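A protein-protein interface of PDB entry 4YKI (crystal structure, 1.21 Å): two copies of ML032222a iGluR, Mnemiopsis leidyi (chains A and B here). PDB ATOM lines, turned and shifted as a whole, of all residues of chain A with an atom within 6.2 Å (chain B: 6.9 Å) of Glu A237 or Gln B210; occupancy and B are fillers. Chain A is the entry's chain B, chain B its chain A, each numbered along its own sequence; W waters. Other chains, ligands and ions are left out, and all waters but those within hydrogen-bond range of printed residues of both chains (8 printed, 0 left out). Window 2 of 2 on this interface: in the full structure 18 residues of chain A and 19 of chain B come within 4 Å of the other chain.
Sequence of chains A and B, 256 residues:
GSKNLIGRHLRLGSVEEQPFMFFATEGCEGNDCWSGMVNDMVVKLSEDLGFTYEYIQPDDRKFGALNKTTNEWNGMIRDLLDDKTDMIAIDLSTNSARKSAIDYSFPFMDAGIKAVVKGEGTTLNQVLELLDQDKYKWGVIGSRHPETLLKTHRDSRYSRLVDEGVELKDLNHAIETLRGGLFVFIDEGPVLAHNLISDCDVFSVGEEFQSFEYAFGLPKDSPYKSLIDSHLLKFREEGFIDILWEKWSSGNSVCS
The backbone NH (N) of Ser B96 sits at hydrogen-bond distance from the side-chain carboxylate (OE1) of Glu A237 (2.9 Å).
The side-chain amide nitrogen (NE2) of Gln B210 is in hydrogen-bond range of the backbone carbonyl oxygen (O) of Glu A237, 3.0 Å away.
OG of Ser B211 sits at hydrogen-bond distance from NE of Arg A236.
O of Phe B212 sits at hydrogen-bond distance from NH2 of Arg A236 (3.4 Å).
The backbone NH of Ala B97 sits at hydrogen-bond distance from the side-chain amide oxygen of Asn B95 (3.3 Å).
ND2 of Asn B95 is in hydrogen-bond range of ND1 of His B145 (3.0 Å).
The backbone NH (N) of Ala B111 is in hydrogen-bond range of the backbone carbonyl oxygen (O) of Phe B212 (2.9 Å).
NZ of Lys A234 lies within salt-bridge range of OE2 of Glu A237 (3.6 Å).
Leu A233 touches Thr B94 (CD1 to OG1, 3.9 Å).
Leu A233 touches Asn B95 (CD2 to O, 3.8 Å).
OG of Ser B96 touches CD of Lys A234, 3.0 Å away.
CA of Asn B95 touches OE1 of Glu A237, 3.2 Å away.
CD2 of Leu B149 touches OE1 of Glu A237, 3.6 Å away.
Leu A232 touches none of the printed residues of chain B.
Printed residues of chain B within 4 Å of Leu A233: Thr B94 (3.9 Å) and Asn B95 (3.8 Å).
Of the printed residues of chain B, Glu A237 touches Asn B95 (3.2 Å), Ser B96 (2.9 Å), Leu B149 (3.6 Å) and Gln B210 (3.0 Å).
Printed residues of chain A within 4 Å of Ser B96: Lys A234 (3.0 Å) and Glu A237 (2.9 Å).
Gln B210 touches one residue of chain A.
Of the printed residues of chain A, Ser B211 touches Arg A236.
The nearest printed residue of chain B that does not touch Glu A237 is Thr B152 (4.01 Å).
Hydrophobic or aromatic side chains of chain A within 4 Å of the printed part of chain B: Leu A233.
Hydrophobic or aromatic side chains of chain B that line the printed part of chain A: Leu B149.
Among the printed residues, no Asp or Glu carboxylate lies within 4 Å of a Lys or Arg side-chain nitrogen of the other chain.
No position is printed for both chains.
Of the 9 pairs that touch across the chains among the printed residues, none has its exchanged pair printed and touching as well.
Water W7 lies within hydrogen-bond range of the side-chain hydroxyl of Thr B152 (2.5 Å) and the side-chain carboxylate of Glu A237 (2.6 Å).
Water W2 bridges O of Thr B94 and OE1 of Glu A237.
Water W5 lies within hydrogen-bond range of the backbone carbonyl oxygen of Arg A236, the backbone NH of Ser B211 and the side-chain amide nitrogen of Gln B210.
Water W8 bridges OD1 of Asp A242 (2.9 Å) and OG of Ser B211 (3.0 Å).
Water W6 lies within hydrogen-bond range of OG of Ser B211 (2.9 Å), NH2 of Arg A236 (3.0 Å), O of Phe B212 (3.1 Å) and O of Ala B111 (3.2 Å).
Water W4 bridges the backbone carbonyl oxygen (O) of Glu A237 (3.4 Å) and the side-chain amide oxygen (OE1) of Gln B210 (3.5 Å).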
ATOM      1  N   LEU A 232      33.748  -5.201  19.707  1.00  0.00           N
ATOM      2  CA  LEU A 232      32.467  -4.654  19.265  1.00  0.00           C
ATOM      3  C   LEU A 232      31.274  -5.476  19.763  1.00  0.00           C
ATOM      4  O   LEU A 232      30.249  -4.918  20.153  1.00  0.00           O
ATOM      5  CB  LEU A 232      32.427  -4.500  17.736  1.00  0.00           C
ATOM      6  CG  LEU A 232      33.327  -3.410  17.165  1.00  0.00           C
ATOM      7  CD1 LEU A 232      33.248  -3.447  15.664  1.00  0.00           C
ATOM      8  CD2 LEU A 232      32.903  -2.051  17.676  1.00  0.00           C
ATOM      9  N   LEU A 233      31.397  -6.800  19.772  1.00  0.00           N
ATOM     10  CA  LEU A 233      30.348  -7.645  20.357  1.00  0.00           C
ATOM     11  C   LEU A 233      30.139  -7.308  21.838  1.00  0.00           C
ATOM     12  O   LEU A 233      29.015  -7.173  22.301  1.00  0.00           O
ATOM     13  CB  LEU A 233      30.683  -9.108  20.142  1.00  0.00           C
ATOM     14  CG  LEU A 233      29.720 -10.133  20.752  1.00  0.00           C
ATOM     15  CD1 LEU A 233      28.255  -9.868  20.477  1.00  0.00           C
ATOM     16  CD2 LEU A 233      30.130 -11.515  20.268  1.00  0.00           C
ATOM     17  N   LYS A 234      31.225  -7.134  22.578  1.00  0.00           N
ATOM     18  CA  LYS A 234      31.112  -6.771  23.984  1.00  0.00           C
ATOM     19  C   LYS A 234      30.416  -5.416  24.157  1.00  0.00           C
ATOM     20  O   LYS A 234      29.537  -5.273  24.990  1.00  0.00           O
ATOM     21  CB  LYS A 234      32.488  -6.773  24.656  1.00  0.00           C
ATOM     22  CG  LYS A 234      32.450  -6.786  26.182  1.00  0.00           C
ATOM     23  CD  LYS A 234      31.785  -8.054  26.714  1.00  0.00           C
ATOM     24  CE  LYS A 234      31.988  -8.264  28.207  1.00  0.00           C
ATOM     25  NZ  LYS A 234      31.084  -9.310  28.748  1.00  0.00           N
ATOM     26  N   PHE A 235      30.796  -4.417  23.363  1.00  0.00           N
ATOM     27  CA  PHE A 235      30.122  -3.117  23.426  1.00  0.00           C
ATOM     28  C   PHE A 235      28.610  -3.307  23.256  1.00  0.00           C
ATOM     29  O   PHE A 235      27.820  -2.715  23.976  1.00  0.00           O
ATOM     30  CB  PHE A 235      30.577  -2.190  22.276  1.00  0.00           C
ATOM     31  CG  PHE A 235      31.961  -1.590  22.407  1.00  0.00           C
ATOM     32  CD1 PHE A 235      32.749  -1.753  23.519  1.00  0.00           C
ATOM     33  CD2 PHE A 235      32.422  -0.803  21.381  1.00  0.00           C
ATOM     34  CE1 PHE A 235      33.996  -1.168  23.588  1.00  0.00           C
ATOM     35  CE2 PHE A 235      33.659  -0.222  21.435  1.00  0.00           C
ATOM     36  CZ  PHE A 235      34.454  -0.389  22.537  1.00  0.00           C
ATOM     37  N   ARG A 236      28.205  -4.149  22.316  1.00  0.00           N
ATOM     38  CA  ARG A 236      26.786  -4.355  22.082  1.00  0.00           C
ATOM     39  C   ARG A 236      26.123  -5.030  23.288  1.00  0.00           C
ATOM     40  O   ARG A 236      25.076  -4.590  23.768  1.00  0.00           O
ATOM     41  CB  ARG A 236      26.582  -5.182  20.821  1.00  0.00           C
ATOM     42  CG  ARG A 236      25.176  -5.258  20.344  1.00  0.00           C
ATOM     43  CD  ARG A 236      25.129  -5.843  18.948  1.00  0.00           C
ATOM     44  NE  ARG A 236      23.768  -6.075  18.516  1.00  0.00           N
ATOM     45  CZ  ARG A 236      23.412  -6.416  17.281  1.00  0.00           C
ATOM     46  NH1 ARG A 236      24.319  -6.571  16.327  1.00  0.00           N
ATOM     47  NH2 ARG A 236      22.146  -6.638  17.014  1.00  0.00           N
ATOM     48  N   GLU A 237      26.755  -6.090  23.777  1.00  0.00           N
ATOM     49  CA  GLU A 237      26.243  -6.867  24.898  1.00  0.00           C
ATOM     50  C   GLU A 237      26.160  -6.053  26.184  1.00  0.00           C
ATOM     51  O   GLU A 237      25.258  -6.252  26.991  1.00  0.00           O
ATOM     52  CB  GLU A 237      27.145  -8.091  25.092  1.00  0.00           C
ATOM     53  CG  GLU A 237      26.728  -9.010  26.232  1.00  0.00           C
ATOM     54  CD  GLU A 237      27.464 -10.322  26.223  1.00  0.00           C
ATOM     55  OE1 GLU A 237      27.409 -11.044  25.222  1.00  0.00           O
ATOM     56  OE2 GLU A 237      28.102 -10.642  27.236  1.00  0.00           O
ATOM     57  N   GLU A 238      27.097  -5.144  26.385  1.00  0.00           N
ATOM     58  CA  GLU A 238      27.096  -4.311  27.579  1.00  0.00           C
ATOM     59  C   GLU A 238      26.143  -3.135  27.499  1.00  0.00           C
ATOM     60  O   GLU A 238      25.943  -2.453  28.496  1.00  0.00           O
ATOM     61  CB  GLU A 238      28.516  -3.836  27.907  1.00  0.00           C
ATOM     62  CG  GLU A 238      29.421  -4.980  28.335  1.00  0.00           C
ATOM     63  CD  GLU A 238      30.850  -4.576  28.562  1.00  0.00           C
ATOM     64  OE1 GLU A 238      31.302  -3.612  27.935  1.00  0.00           O
ATOM     65  OE2 GLU A 238      31.526  -5.251  29.365  1.00  0.00           O
ATOM     66  N   GLY A 239      25.553  -2.897  26.335  1.00  0.00           N
ATOM     67  CA  GLY A 239      24.607  -1.808  26.165  1.00  0.00           C
ATOM     68  C   GLY A 239      25.235  -0.507  25.704  1.00  0.00           C
ATOM     69  O   GLY A 239      24.545   0.513  25.605  1.00  0.00           O
ATOM     70  N   PHE A 240      26.536  -0.539  25.442  1.00  0.00           N
ATOM     71  CA  PHE A 240      27.274   0.673  25.098  1.00  0.00           C
ATOM     72  C   PHE A 240      26.827   1.270  23.761  1.00  0.00           C
ATOM     73  O   PHE A 240      26.725   2.488  23.622  1.00  0.00           O
ATOM     74  CB  PHE A 240      28.769   0.361  25.093  1.00  0.00           C
ATOM     75  CG  PHE A 240      29.671   1.560  24.903  1.00  0.00           C
ATOM     76  CD1 PHE A 240      29.577   2.685  25.716  1.00  0.00           C
ATOM     77  CD2 PHE A 240      30.661   1.528  23.941  1.00  0.00           C
ATOM     78  CE1 PHE A 240      30.426   3.758  25.542  1.00  0.00           C
ATOM     79  CE2 PHE A 240      31.525   2.602  23.770  1.00  0.00           C
ATOM     80  CZ  PHE A 240      31.410   3.710  24.580  1.00  0.00           C
ATOM     81  N   ASP A 242      23.854   1.115  22.378  1.00  0.00           N
ATOM     82  CA  ASP A 242      22.560   1.753  22.581  1.00  0.00           C
ATOM     83  C   ASP A 242      22.718   3.065  23.358  1.00  0.00           C
ATOM     84  O   ASP A 242      22.068   4.056  23.040  1.00  0.00           O
ATOM     85  CB  ASP A 242      21.590   0.813  23.317  1.00  0.00           C
ATOM     86  CG  ASP A 242      21.075  -0.331  22.452  1.00  0.00           C
ATOM     87  OD1 ASP A 242      21.111  -0.236  21.223  1.00  0.00           O
ATOM     88  OD2 ASP A 242      20.586  -1.324  23.015  1.00  0.00           O
ATOM     89  N   THR B  94      24.595 -14.593  19.635  1.00  0.00           N
ATOM     90  CA  THR B  94      25.913 -14.027  19.870  1.00  0.00           C
ATOM     91  C   THR B  94      26.069 -13.561  21.316  1.00  0.00           C
ATOM     92  O   THR B  94      25.292 -12.749  21.798  1.00  0.00           O
ATOM     93  CB  THR B  94      26.220 -12.875  18.895  1.00  0.00           C
ATOM     94  OG1 THR B  94      25.224 -11.844  19.014  1.00  0.00           O
ATOM     95  CG2 THR B  94      26.278 -13.375  17.461  1.00  0.00           C
ATOM     96  N   ASN B  95      27.082 -14.089  22.004  1.00  0.00           N
ATOM     97  CA  ASN B  95      27.460 -13.588  23.316  1.00  0.00           C
ATOM     98  C   ASN B  95      28.970 -13.662  23.481  1.00  0.00           C
ATOM     99  O   ASN B  95      29.661 -14.392  22.766  1.00  0.00           O
ATOM    100  CB  ASN B  95      26.678 -14.240  24.482  1.00  0.00           C
ATOM    101  CG  ASN B  95      26.948 -15.730  24.653  1.00  0.00           C
ATOM    102  OD1 ASN B  95      28.082 -16.135  24.854  1.00  0.00           O
ATOM    103  ND2 ASN B  95      25.890 -16.529  24.689  1.00  0.00           N
ATOM    104  N   SER B  96      29.479 -12.858  24.403  1.00  0.00           N
ATOM    105  CA  SER B  96      30.914 -12.716  24.588  1.00  0.00           C
ATOM    106  C   SER B  96      31.557 -14.008  25.109  1.00  0.00           C
ATOM    107  O   SER B  96      32.671 -14.332  24.723  1.00  0.00           O
ATOM    108  CB  SER B  96      31.213 -11.547  25.524  1.00  0.00           C
ATOM    109  OG  SER B  96      30.878 -10.298  24.927  1.00  0.00           O
ATOM    110  N   ALA B  97      30.847 -14.774  25.937  1.00  0.00           N
ATOM    111  CA  ALA B  97      31.385 -16.044  26.447  1.00  0.00           C
ATOM    112  C   ALA B  97      31.695 -16.977  25.277  1.00  0.00           C
ATOM    113  O   ALA B  97      32.782 -17.502  25.160  1.00  0.00           O
ATOM    114  CB  ALA B  97      30.429 -16.693  27.422  1.00  0.00           C
ATOM    115  N   ALA B 111      18.001  -9.900  17.674  1.00  0.00           N
ATOM    116  CA  ALA B 111      17.133 -10.488  18.688  1.00  0.00           C
ATOM    117  C   ALA B 111      17.387  -9.831  20.051  1.00  0.00           C
ATOM    118  O   ALA B 111      18.443  -9.232  20.283  1.00  0.00           O
ATOM    119  CB  ALA B 111      17.344 -12.016  18.747  1.00  0.00           C
ATOM    120  N   GLY B 112      16.405  -9.955  20.943  1.00  0.00           N
ATOM    121  CA  GLY B 112      16.512  -9.493  22.317  1.00  0.00           C
ATOM    122  C   GLY B 112      15.985 -10.530  23.275  1.00  0.00           C
ATOM    123  O   GLY B 112      15.393 -11.526  22.859  1.00  0.00           O
ATOM    124  N   ILE B 113      16.201 -10.292  24.563  1.00  0.00           N
ATOM    125  CA  ILE B 113      15.619 -11.117  25.609  1.00  0.00           C
ATOM    126  C   ILE B 113      14.215 -10.616  25.908  1.00  0.00           C
ATOM    127  O   ILE B 113      13.990  -9.407  26.036  1.00  0.00           O
ATOM    128  CB  ILE B 113      16.477 -11.085  26.902  1.00  0.00           C
ATOM    129  CG1 ILE B 113      17.893 -11.593  26.612  1.00  0.00           C
ATOM    130  CG2 ILE B 113      15.831 -11.905  28.023  1.00  0.00           C
ATOM    131  CD1 ILE B 113      17.953 -12.998  26.027  1.00  0.00           C
ATOM    132  N   HIS B 145      21.634 -19.355  25.731  1.00  0.00           N
ATOM    133  CA  HIS B 145      22.052 -17.968  25.718  1.00  0.00           C
ATOM    134  C   HIS B 145      21.393 -17.043  26.761  1.00  0.00           C
ATOM    135  O   HIS B 145      22.118 -16.309  27.410  1.00  0.00           O
ATOM    136  CB  HIS B 145      21.903 -17.441  24.281  1.00  0.00           C
ATOM    137  CG  HIS B 145      22.013 -15.965  24.139  1.00  0.00           C
ATOM    138  ND1 HIS B 145      23.212 -15.291  24.081  1.00  0.00           N
ATOM    139  CD2 HIS B 145      21.039 -15.045  23.962  1.00  0.00           C
ATOM    140  CE1 HIS B 145      22.959 -14.007  23.896  1.00  0.00           C
ATOM    141  NE2 HIS B 145      21.652 -13.834  23.807  1.00  0.00           N
ATOM    142  N   THR B 148      23.029 -17.423  30.048  1.00  0.00           N
ATOM    143  CA  THR B 148      24.366 -16.838  29.991  1.00  0.00           C
ATOM    144  C   THR B 148      24.350 -15.325  30.096  1.00  0.00           C
ATOM    145  O   THR B 148      25.126 -14.767  30.868  1.00  0.00           O
ATOM    146  CB  THR B 148      25.102 -17.269  28.712  1.00  0.00           C
ATOM    147  OG1 THR B 148      25.418 -18.662  28.810  1.00  0.00           O
ATOM    148  CG2 THR B 148      26.397 -16.465  28.489  1.00  0.00           C
ATOM    149  N   LEU B 149      23.481 -14.662  29.346  1.00  0.00           N
ATOM    150  CA  LEU B 149      23.397 -13.205  29.442  1.00  0.00           C
ATOM    151  C   LEU B 149      22.958 -12.719  30.814  1.00  0.00           C
ATOM    152  O   LEU B 149      23.503 -11.755  31.341  1.00  0.00           O
ATOM    153  CB  LEU B 149      22.456 -12.624  28.401  1.00  0.00           C
ATOM    154  CG  LEU B 149      22.893 -12.596  26.946  1.00  0.00           C
ATOM    155  CD1 LEU B 149      21.951 -11.647  26.203  1.00  0.00           C
ATOM    156  CD2 LEU B 149      24.341 -12.162  26.783  1.00  0.00           C
ATOM    157  N   LEU B 150      21.992 -13.385  31.423  1.00  0.00           N
ATOM    158  CA  LEU B 150      21.560 -12.941  32.738  1.00  0.00           C
ATOM    159  C   LEU B 150      22.644 -13.189  33.780  1.00  0.00           C
ATOM    160  O   LEU B 150      22.827 -12.364  34.673  1.00  0.00           O
ATOM    161  CB  LEU B 150      20.244 -13.597  33.145  1.00  0.00           C
ATOM    162  CG  LEU B 150      18.990 -12.845  32.658  1.00  0.00           C
ATOM    163  CD1 LEU B 150      18.918 -12.717  31.141  1.00  0.00           C
ATOM    164  CD2 LEU B 150      17.722 -13.511  33.217  1.00  0.00           C
ATOM    165  N   THR B 152      25.840 -13.151  33.272  1.00  0.00           N
ATOM    166  CA  THR B 152      26.994 -12.282  33.039  1.00  0.00           C
ATOM    167  C   THR B 152      26.624 -10.783  33.083  1.00  0.00           C
ATOM    168  O   THR B 152      27.523  -9.933  33.062  1.00  0.00           O
ATOM    169  CB  THR B 152      27.762 -12.683  31.734  1.00  0.00           C
ATOM    170  OG1 THR B 152      26.936 -12.510  30.583  1.00  0.00           O
ATOM    171  CG2 THR B 152      28.224 -14.144  31.796  1.00  0.00           C
ATOM    172  N   HIS B 153      25.341 -10.446  33.197  1.00  0.00           N
ATOM    173  CA  HIS B 153      24.869  -9.057  33.285  1.00  0.00           C
ATOM    174  C   HIS B 153      25.538  -8.318  34.439  1.00  0.00           C
ATOM    175  O   HIS B 153      25.854  -8.933  35.468  1.00  0.00           O
ATOM    176  CB  HIS B 153      23.340  -9.018  33.467  1.00  0.00           C
ATOM    177  CG  HIS B 153      22.697  -7.700  33.140  1.00  0.00           C
ATOM    178  ND1 HIS B 153      22.773  -6.597  33.967  1.00  0.00           N
ATOM    179  CD2 HIS B 153      21.933  -7.323  32.086  1.00  0.00           C
ATOM    180  CE1 HIS B 153      22.096  -5.598  33.431  1.00  0.00           C
ATOM    181  NE2 HIS B 153      21.573  -6.015  32.290  1.00  0.00           N
ATOM    182  N   ARG B 154      25.742  -7.010  34.246  1.00  0.00           N
ATOM    183  CA  ARG B 154      26.426  -6.152  35.216  1.00  0.00           C
ATOM    184  C   ARG B 154      25.699  -6.111  36.539  1.00  0.00           C
ATOM    185  O   ARG B 154      26.335  -6.082  37.602  1.00  0.00           O
ATOM    186  CB  ARG B 154      26.572  -4.715  34.673  1.00  0.00           C
ATOM    187  CG  ARG B 154      25.259  -3.970  34.411  1.00  0.00           C
ATOM    188  CD  ARG B 154      25.513  -2.534  33.935  1.00  0.00           C
ATOM    189  NE  ARG B 154      24.286  -1.877  33.507  1.00  0.00           N
ATOM    190  CZ  ARG B 154      23.399  -1.335  34.342  1.00  0.00           C
ATOM    191  NH1 ARG B 154      23.603  -1.367  35.656  1.00  0.00           N
ATOM    192  NH2 ARG B 154      22.301  -0.757  33.870  1.00  0.00           N
ATOM    193  N   TYR B 158      20.260  -9.936  38.129  1.00  0.00           N
ATOM    194  CA  TYR B 158      19.917 -10.874  37.050  1.00  0.00           C
ATOM    195  C   TYR B 158      20.486 -12.270  37.310  1.00  0.00           C
ATOM    196  O   TYR B 158      19.856 -13.265  36.966  1.00  0.00           O
ATOM    197  CB  TYR B 158      20.309 -10.337  35.663  1.00  0.00           C
ATOM    198  CG  TYR B 158      19.396  -9.213  35.201  1.00  0.00           C
ATOM    199  CD1 TYR B 158      18.117  -9.467  34.734  1.00  0.00           C
ATOM    200  CD2 TYR B 158      19.817  -7.895  35.254  1.00  0.00           C
ATOM    201  CE1 TYR B 158      17.273  -8.437  34.333  1.00  0.00           C
ATOM    202  CE2 TYR B 158      18.979  -6.859  34.853  1.00  0.00           C
ATOM    203  CZ  TYR B 158      17.716  -7.143  34.394  1.00  0.00           C
ATOM    204  OH  TYR B 158      16.882  -6.121  34.001  1.00  0.00           O
ATOM    205  N   GLU B 208      11.454  -5.825  25.913  1.00  0.00           N
ATOM    206  CA  GLU B 208      12.640  -6.601  25.575  1.00  0.00           C
ATOM    207  C   GLU B 208      13.890  -5.862  26.033  1.00  0.00           C
ATOM    208  O   GLU B 208      13.909  -4.627  26.074  1.00  0.00           O
ATOM    209  CB  GLU B 208      12.685  -6.888  24.073  1.00  0.00           C
ATOM    210  CG  GLU B 208      11.578  -7.845  23.642  1.00  0.00           C
ATOM    211  CD  GLU B 208      11.736  -8.386  22.235  1.00  0.00           C
ATOM    212  OE1 GLU B 208      12.844  -8.284  21.668  1.00  0.00           O
ATOM    213  OE2 GLU B 208      10.740  -8.931  21.705  1.00  0.00           O
ATOM    214  N   PHE B 209      14.930  -6.604  26.405  1.00  0.00           N
ATOM    215  CA  PHE B 209      16.188  -6.008  26.817  1.00  0.00           C
ATOM    216  C   PHE B 209      17.321  -6.876  26.294  1.00  0.00           C
ATOM    217  O   PHE B 209      17.109  -8.063  26.007  1.00  0.00           O
ATOM    218  CB  PHE B 209      16.260  -5.831  28.349  1.00  0.00           C
ATOM    219  CG  PHE B 209      16.093  -7.110  29.141  1.00  0.00           C
ATOM    220  CD1 PHE B 209      14.849  -7.704  29.273  1.00  0.00           C
ATOM    221  CD2 PHE B 209      17.170  -7.685  29.793  1.00  0.00           C
ATOM    222  CE1 PHE B 209      14.688  -8.868  30.005  1.00  0.00           C
ATOM    223  CE2 PHE B 209      17.005  -8.862  30.532  1.00  0.00           C
ATOM    224  CZ  PHE B 209      15.765  -9.436  30.638  1.00  0.00           C
ATOM    225  N   GLN B 210      18.516  -6.298  26.218  1.00  0.00           N
ATOM    226  CA  GLN B 210      19.697  -6.888  25.575  1.00  0.00           C
ATOM    227  C   GLN B 210      19.572  -6.881  24.047  1.00  0.00           C
ATOM    228  O   GLN B 210      18.492  -7.077  23.485  1.00  0.00           O
ATOM    229  CB  GLN B 210      20.032  -8.298  26.080  1.00  0.00           C
ATOM    230  CG  GLN B 210      20.394  -8.408  27.564  1.00  0.00           C
ATOM    231  CD  GLN B 210      21.756  -7.820  27.936  1.00  0.00           C
ATOM    232  OE1 GLN B 210      21.926  -7.341  29.053  1.00  0.00           O
ATOM    233  NE2 GLN B 210      22.725  -7.851  27.022  1.00  0.00           N
ATOM    234  N   SER B 211      20.693  -6.628  23.395  1.00  0.00           N
ATOM    235  CA  SER B 211      20.771  -6.601  21.949  1.00  0.00           C
ATOM    236  C   SER B 211      21.796  -7.611  21.465  1.00  0.00           C
ATOM    237  O   SER B 211      22.964  -7.520  21.849  1.00  0.00           O
ATOM    238  CB  SER B 211      21.189  -5.202  21.494  1.00  0.00           C
ATOM    239  OG  SER B 211      21.411  -5.155  20.100  1.00  0.00           O
ATOM    240  N   PHE B 212      21.362  -8.565  20.634  1.00  0.00           N
ATOM    241  CA  PHE B 212      22.268  -9.557  20.079  1.00  0.00           C
ATOM    242  C   PHE B 212      21.789 -10.024  18.709  1.00  0.00           C
ATOM    243  O   PHE B 212      20.804  -9.517  18.188  1.00  0.00           O
ATOM    244  CB  PHE B 212      22.493 -10.719  21.053  1.00  0.00           C
ATOM    245  CG  PHE B 212      21.236 -11.455  21.437  1.00  0.00           C
ATOM    246  CD1 PHE B 212      20.429 -10.998  22.475  1.00  0.00           C
ATOM    247  CD2 PHE B 212      20.827 -12.578  20.741  1.00  0.00           C
ATOM    248  CE1 PHE B 212      19.262 -11.660  22.821  1.00  0.00           C
ATOM    249  CE2 PHE B 212      19.654 -13.250  21.091  1.00  0.00           C
ATOM    250  CZ  PHE B 212      18.870 -12.766  22.126  1.00  0.00           C
HETATM  251  O   HOH W   1      28.555 -13.500  27.567  1.00  0.00           O
HETATM  252  O   HOH W   2      25.290 -10.585  23.505  1.00  0.00           O
HETATM  253  O   HOH W   3      23.833  -0.706  30.372  1.00  0.00           O
HETATM  254  O   HOH W   4      22.484  -4.306  27.509  1.00  0.00           O
HETATM  255  O   HOH W   5      22.621  -5.157  24.951  1.00  0.00           O
HETATM  256  O   HOH W   6      19.536  -6.718  18.539  1.00  0.00           O
HETATM  257  O   HOH W   7      27.280 -10.245  29.665  1.00  0.00           O
HETATM  258  O   HOH W   8      22.672  -2.483  20.311  1.00  0.00           O
